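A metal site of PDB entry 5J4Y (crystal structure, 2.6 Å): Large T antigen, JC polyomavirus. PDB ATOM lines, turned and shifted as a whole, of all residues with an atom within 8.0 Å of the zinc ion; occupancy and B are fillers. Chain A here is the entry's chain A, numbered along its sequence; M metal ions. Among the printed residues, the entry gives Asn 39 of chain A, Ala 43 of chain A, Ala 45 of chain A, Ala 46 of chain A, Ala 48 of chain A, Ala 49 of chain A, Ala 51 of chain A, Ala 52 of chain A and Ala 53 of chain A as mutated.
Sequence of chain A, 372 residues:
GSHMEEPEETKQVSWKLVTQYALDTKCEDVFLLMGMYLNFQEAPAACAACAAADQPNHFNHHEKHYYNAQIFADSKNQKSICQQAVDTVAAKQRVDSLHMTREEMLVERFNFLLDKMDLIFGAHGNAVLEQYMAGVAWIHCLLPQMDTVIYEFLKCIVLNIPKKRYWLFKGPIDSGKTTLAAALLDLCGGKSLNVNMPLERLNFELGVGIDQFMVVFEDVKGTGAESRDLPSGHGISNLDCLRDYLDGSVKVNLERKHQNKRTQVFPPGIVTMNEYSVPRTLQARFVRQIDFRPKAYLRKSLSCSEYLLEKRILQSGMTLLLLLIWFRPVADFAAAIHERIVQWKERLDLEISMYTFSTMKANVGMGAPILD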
ATOM      1  N   ASN A  39     -17.930  22.303  19.734  1.00  0.00           N
ATOM      2  CA  ASN A  39     -16.857  22.977  20.489  1.00  0.00           C
ATOM      3  C   ASN A  39     -17.104  23.060  22.000  1.00  0.00           C
ATOM      4  O   ASN A  39     -16.184  23.378  22.742  1.00  0.00           O
ATOM      5  CB  ASN A  39     -16.565  24.356  19.904  1.00  0.00           C
ATOM      6  CG  ASN A  39     -15.755  24.343  18.627  1.00  0.00           C
ATOM      7  OD1 ASN A  39     -15.349  23.293  18.104  1.00  0.00           O
ATOM      8  ND2 ASN A  39     -15.492  25.516  18.094  1.00  0.00           N
ATOM      9  N   PHE A  40     -18.333  22.752  22.439  1.00  0.00           N
ATOM     10  CA  PHE A  40     -18.750  22.726  23.835  1.00  0.00           C
ATOM     11  C   PHE A  40     -18.374  21.414  24.546  1.00  0.00           C
ATOM     12  O   PHE A  40     -18.576  21.310  25.760  1.00  0.00           O
ATOM     13  CB  PHE A  40     -20.274  22.887  23.940  1.00  0.00           C
ATOM     14  CG  PHE A  40     -20.927  24.171  23.490  1.00  0.00           C
ATOM     15  CD1 PHE A  40     -20.371  25.404  23.835  1.00  0.00           C
ATOM     16  CD2 PHE A  40     -22.156  24.158  22.833  1.00  0.00           C
ATOM     17  CE1 PHE A  40     -21.002  26.593  23.464  1.00  0.00           C
ATOM     18  CE2 PHE A  40     -22.782  25.346  22.475  1.00  0.00           C
ATOM     19  CZ  PHE A  40     -22.207  26.552  22.788  1.00  0.00           C
ATOM     20  N   GLN A  41     -17.875  20.412  23.814  1.00  0.00           N
ATOM     21  CA  GLN A  41     -17.583  19.093  24.383  1.00  0.00           C
ATOM     22  C   GLN A  41     -16.298  19.064  25.254  1.00  0.00           C
ATOM     23  O   GLN A  41     -16.153  18.162  26.087  1.00  0.00           O
ATOM     24  CB  GLN A  41     -17.572  17.993  23.313  1.00  0.00           C
ATOM     25  CG  GLN A  41     -16.373  18.005  22.384  1.00  0.00           C
ATOM     26  CD  GLN A  41     -16.195  16.709  21.659  1.00  0.00           C
ATOM     27  OE1 GLN A  41     -16.336  16.629  20.435  1.00  0.00           O
ATOM     28  NE2 GLN A  41     -15.836  15.657  22.393  1.00  0.00           N
ATOM     29  N   GLU A  42     -15.368  20.022  25.046  1.00  0.00           N
ATOM     30  CA  GLU A  42     -14.140  20.116  25.830  1.00  0.00           C
ATOM     31  C   GLU A  42     -14.436  20.678  27.216  1.00  0.00           C
ATOM     32  O   GLU A  42     -15.398  21.444  27.364  1.00  0.00           O
ATOM     33  CB  GLU A  42     -13.057  20.925  25.109  1.00  0.00           C
ATOM     34  CG  GLU A  42     -13.526  22.224  24.470  1.00  0.00           C
ATOM     35  CD  GLU A  42     -12.833  22.516  23.154  1.00  0.00           C
ATOM     36  OE1 GLU A  42     -11.879  23.338  23.147  1.00  0.00           O
ATOM     37  OE2 GLU A  42     -13.217  21.904  22.127  1.00  0.00           O
ATOM     38  N   ALA A  43     -13.635  20.267  28.241  1.00  0.00           N
ATOM     39  CA  ALA A  43     -13.773  20.682  29.653  1.00  0.00           C
ATOM     40  C   ALA A  43     -13.644  22.200  29.801  1.00  0.00           C
ATOM     41  O   ALA A  43     -12.683  22.758  29.280  1.00  0.00           O
ATOM     42  CB  ALA A  43     -12.732  19.975  30.516  1.00  0.00           C
ATOM     43  N   PRO A  44     -14.610  22.885  30.458  1.00  0.00           N
ATOM     44  CA  PRO A  44     -14.505  24.351  30.577  1.00  0.00           C
ATOM     45  C   PRO A  44     -13.374  24.812  31.500  1.00  0.00           C
ATOM     46  O   PRO A  44     -12.942  25.953  31.379  1.00  0.00           O
ATOM     47  CB  PRO A  44     -15.879  24.768  31.126  1.00  0.00           C
ATOM     48  CG  PRO A  44     -16.754  23.554  31.023  1.00  0.00           C
ATOM     49  CD  PRO A  44     -15.836  22.382  31.113  1.00  0.00           C
ATOM     50  N   ALA A  45     -12.878  23.913  32.381  1.00  0.00           N
ATOM     51  CA  ALA A  45     -11.778  24.169  33.319  1.00  0.00           C
ATOM     52  C   ALA A  45     -10.392  24.100  32.637  1.00  0.00           C
ATOM     53  O   ALA A  45      -9.418  24.655  33.161  1.00  0.00           O
ATOM     54  CB  ALA A  45     -11.839  23.198  34.489  1.00  0.00           C
ATOM     55  N   ALA A  46     -10.316  23.417  31.467  1.00  0.00           N
ATOM     56  CA  ALA A  46      -9.099  23.239  30.670  1.00  0.00           C
ATOM     57  C   ALA A  46      -9.246  23.794  29.230  1.00  0.00           C
ATOM     58  O   ALA A  46      -8.316  23.693  28.430  1.00  0.00           O
ATOM     59  CB  ALA A  46      -8.700  21.767  30.631  1.00  0.00           C
ATOM     60  N   CYS A  47     -10.423  24.390  28.918  1.00  0.00           N
ATOM     61  CA  CYS A  47     -10.736  24.974  27.614  1.00  0.00           C
ATOM     62  C   CYS A  47     -10.005  26.291  27.391  1.00  0.00           C
ATOM     63  O   CYS A  47      -9.873  27.096  28.317  1.00  0.00           O
ATOM     64  CB  CYS A  47     -12.244  25.137  27.442  1.00  0.00           C
ATOM     65  SG  CYS A  47     -12.775  25.581  25.766  1.00  0.00           S
ATOM     66  N   ALA A  48      -9.561  26.520  26.143  1.00  0.00           N
ATOM     67  CA  ALA A  48      -8.857  27.735  25.734  1.00  0.00           C
ATOM     68  C   ALA A  48      -9.824  28.892  25.449  1.00  0.00           C
ATOM     69  O   ALA A  48      -9.607  29.998  25.931  1.00  0.00           O
ATOM     70  CB  ALA A  48      -7.983  27.455  24.520  1.00  0.00           C
ATOM     71  N   ALA A  49     -10.920  28.622  24.678  1.00  0.00           N
ATOM     72  CA  ALA A  49     -11.944  29.608  24.304  1.00  0.00           C
ATOM     73  C   ALA A  49     -12.833  30.056  25.484  1.00  0.00           C
ATOM     74  O   ALA A  49     -13.510  31.081  25.376  1.00  0.00           O
ATOM     75  CB  ALA A  49     -12.792  29.063  23.160  1.00  0.00           C
ATOM     76  N   CYS A  50     -12.822  29.281  26.597  1.00  0.00           N
ATOM     77  CA  CYS A  50     -13.589  29.565  27.811  1.00  0.00           C
ATOM     78  C   CYS A  50     -12.945  30.704  28.601  1.00  0.00           C
ATOM     79  O   CYS A  50     -13.614  31.705  28.883  1.00  0.00           O
ATOM     80  CB  CYS A  50     -13.750  28.311  28.659  1.00  0.00           C
ATOM     81  SG  CYS A  50     -15.476  27.804  28.947  1.00  0.00           S
ATOM     82  N   ALA A  51     -11.640  30.550  28.941  1.00  0.00           N
ATOM     83  CA  ALA A  51     -10.825  31.499  29.711  1.00  0.00           C
ATOM     84  C   ALA A  51     -10.483  32.789  28.946  1.00  0.00           C
ATOM     85  O   ALA A  51     -10.344  33.840  29.569  1.00  0.00           O
ATOM     86  CB  ALA A  51      -9.552  30.834  30.194  1.00  0.00           C
ATOM     87  N   ALA A  52     -10.333  32.695  27.609  1.00  0.00           N
ATOM     88  CA  ALA A  52     -10.023  33.827  26.729  1.00  0.00           C
ATOM     89  C   ALA A  52     -11.222  34.759  26.539  1.00  0.00           C
ATOM     90  O   ALA A  52     -11.033  35.945  26.278  1.00  0.00           O
ATOM     91  CB  ALA A  52      -9.520  33.335  25.378  1.00  0.00           C
ATOM     92  N   ALA A  53     -12.462  34.204  26.680  1.00  0.00           N
ATOM     93  CA  ALA A  53     -13.766  34.875  26.543  1.00  0.00           C
ATOM     94  C   ALA A  53     -13.892  35.673  25.233  1.00  0.00           C
ATOM     95  O   ALA A  53     -14.088  36.899  25.236  1.00  0.00           O
ATOM     96  CB  ALA A  53     -14.060  35.751  27.768  1.00  0.00           C
ATOM     97  N   GLN A  55     -15.991  34.430  22.367  1.00  0.00           N
ATOM     98  CA  GLN A  55     -17.354  34.301  21.850  1.00  0.00           C
ATOM     99  C   GLN A  55     -18.390  34.267  22.994  1.00  0.00           C
ATOM    100  O   GLN A  55     -18.156  33.518  23.956  1.00  0.00           O
ATOM    101  CB  GLN A  55     -17.485  33.056  20.947  1.00  0.00           C
ATOM    102  N   HIS A  58     -20.190  30.994  23.508  1.00  0.00           N
ATOM    103  CA  HIS A  58     -19.276  29.933  23.928  1.00  0.00           C
ATOM    104  C   HIS A  58     -19.219  29.753  25.451  1.00  0.00           C
ATOM    105  O   HIS A  58     -19.627  28.701  25.912  1.00  0.00           O
ATOM    106  CB  HIS A  58     -17.876  30.110  23.325  1.00  0.00           C
ATOM    107  CG  HIS A  58     -16.982  28.918  23.564  1.00  0.00           C
ATOM    108  ND1 HIS A  58     -16.874  27.901  22.632  1.00  0.00           N
ATOM    109  CD2 HIS A  58     -16.203  28.632  24.633  1.00  0.00           C
ATOM    110  CE1 HIS A  58     -16.026  27.030  23.157  1.00  0.00           C
ATOM    111  NE2 HIS A  58     -15.600  27.420  24.358  1.00  0.00           N
ATOM    112  N   PHE A  59     -18.684  30.739  26.237  1.00  0.00           N
ATOM    113  CA  PHE A  59     -18.521  30.606  27.692  1.00  0.00           C
ATOM    114  C   PHE A  59     -19.823  30.642  28.522  1.00  0.00           C
ATOM    115  O   PHE A  59     -19.879  29.984  29.568  1.00  0.00           O
ATOM    116  CB  PHE A  59     -17.499  31.618  28.249  1.00  0.00           C
ATOM    117  CG  PHE A  59     -17.806  33.081  28.047  1.00  0.00           C
ATOM    118  CD1 PHE A  59     -17.298  33.768  26.949  1.00  0.00           C
ATOM    119  CD2 PHE A  59     -18.534  33.806  28.987  1.00  0.00           C
ATOM    120  CE1 PHE A  59     -17.576  35.133  26.761  1.00  0.00           C
ATOM    121  CE2 PHE A  59     -18.806  35.160  28.804  1.00  0.00           C
ATOM    122  CZ  PHE A  59     -18.323  35.817  27.693  1.00  0.00           C
ATOM    123  N   ASN A  60     -20.834  31.412  28.081  1.00  0.00           N
ATOM    124  CA  ASN A  60     -22.118  31.552  28.791  1.00  0.00           C
ATOM    125  C   ASN A  60     -23.002  30.293  28.651  1.00  0.00           C
ATOM    126  O   ASN A  60     -23.803  29.983  29.535  1.00  0.00           O
ATOM    127  CB  ASN A  60     -22.884  32.772  28.279  1.00  0.00           C
ATOM    128  CG  ASN A  60     -22.190  34.090  28.512  1.00  0.00           C
ATOM    129  OD1 ASN A  60     -21.963  34.518  29.648  1.00  0.00           O
ATOM    130  ND2 ASN A  60     -21.888  34.793  27.421  1.00  0.00           N
ATOM    131  N   HIS A  61     -22.838  29.600  27.520  1.00  0.00           N
ATOM    132  CA  HIS A  61     -23.579  28.408  27.165  1.00  0.00           C
ATOM    133  C   HIS A  61     -22.746  27.151  27.398  1.00  0.00           C
ATOM    134  O   HIS A  61     -23.304  26.056  27.430  1.00  0.00           O
ATOM    135  CB  HIS A  61     -23.973  28.488  25.687  1.00  0.00           C
ATOM    136  CG  HIS A  61     -24.753  29.713  25.306  1.00  0.00           C
ATOM    137  ND1 HIS A  61     -26.133  29.737  25.366  1.00  0.00           N
ATOM    138  CD2 HIS A  61     -24.313  30.906  24.843  1.00  0.00           C
ATOM    139  CE1 HIS A  61     -26.487  30.931  24.936  1.00  0.00           C
ATOM    140  NE2 HIS A  61     -25.425  31.674  24.608  1.00  0.00           N
ATOM    141  N   HIS A  62     -21.406  27.290  27.539  1.00  0.00           N
ATOM    142  CA  HIS A  62     -20.500  26.148  27.728  1.00  0.00           C
ATOM    143  C   HIS A  62     -20.909  25.254  28.875  1.00  0.00           C
ATOM    144  O   HIS A  62     -20.951  24.046  28.699  1.00  0.00           O
ATOM    145  CB  HIS A  62     -19.034  26.568  27.884  1.00  0.00           C
ATOM    146  CG  HIS A  62     -18.069  25.541  27.378  1.00  0.00           C
ATOM    147  ND1 HIS A  62     -17.225  25.808  26.312  1.00  0.00           N
ATOM    148  CD2 HIS A  62     -17.847  24.273  27.803  1.00  0.00           C
ATOM    149  CE1 HIS A  62     -16.514  24.706  26.132  1.00  0.00           C
ATOM    150  NE2 HIS A  62     -16.856  23.758  27.001  1.00  0.00           N
ATOM    151  N   GLU A  63     -21.223  25.849  30.031  1.00  0.00           N
ATOM    152  CA  GLU A  63     -21.659  25.092  31.195  1.00  0.00           C
ATOM    153  C   GLU A  63     -23.006  24.421  30.916  1.00  0.00           C
ATOM    154  O   GLU A  63     -23.108  23.206  31.098  1.00  0.00           O
ATOM    155  CB  GLU A  63     -21.707  26.003  32.445  1.00  0.00           C
ATOM    156  CG  GLU A  63     -21.014  25.407  33.658  1.00  0.00           C
ATOM    157  CD  GLU A  63     -19.541  25.068  33.485  1.00  0.00           C
ATOM    158  OE1 GLU A  63     -18.698  25.999  33.554  1.00  0.00           O
ATOM    159  OE2 GLU A  63     -19.232  23.873  33.285  1.00  0.00           O
ATOM    160  N   TYR A  66     -22.343  21.653  27.888  1.00  0.00           N
ATOM    161  CA  TYR A  66     -21.151  20.800  27.999  1.00  0.00           C
ATOM    162  C   TYR A  66     -21.448  19.289  27.956  1.00  0.00           C
ATOM    163  O   TYR A  66     -20.874  18.601  27.108  1.00  0.00           O
ATOM    164  CB  TYR A  66     -20.302  21.167  29.245  1.00  0.00           C
ATOM    165  CG  TYR A  66     -19.197  20.191  29.583  1.00  0.00           C
ATOM    166  CD1 TYR A  66     -18.103  20.017  28.740  1.00  0.00           C
ATOM    167  CD2 TYR A  66     -19.243  19.440  30.762  1.00  0.00           C
ATOM    168  CE1 TYR A  66     -17.095  19.109  29.047  1.00  0.00           C
ATOM    169  CE2 TYR A  66     -18.242  18.520  31.071  1.00  0.00           C
ATOM    170  CZ  TYR A  66     -17.174  18.346  30.200  1.00  0.00           C
ATOM    171  OH  TYR A  66     -16.172  17.456  30.495  1.00  0.00           O
HETATM  172 ZN    ZN M   1     -15.323  27.011  26.843  1.00  0.00          ZN
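SG of Cys 47 sits at hydrogen-bond distance from N of Cys 50. SG of Cys 47 is in hydrogen-bond range of OE1 of Glu 42. A ring nitrogen (NE2) of His 62 lies within hydrogen-bond range of the backbone carbonyl oxygen of Glu 42 (2.8 Å). SG of Cys 47 sits close to N of Ala 49 (3.7 Å). The backbone carbonyl oxygen of Phe 40 is in hydrogen-bond range of a ring nitrogen (NE2) of His 62 (3.2 Å). A ring nitrogen (NE2) of His 58 sits close to the side-chain sulfur of Cys 47 (3.7 Å).
SG of Cys 47 touches the zinc ion, at 3.1 Å.
SG of Cys 50 is bound to the zinc ion. The zinc ion is bound by ND1 of His 62, 2.3 Å away. NE2 of His 58 binds the zinc ion, at 2.5 Å. The zinc ion has three donor atoms within binding distance.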
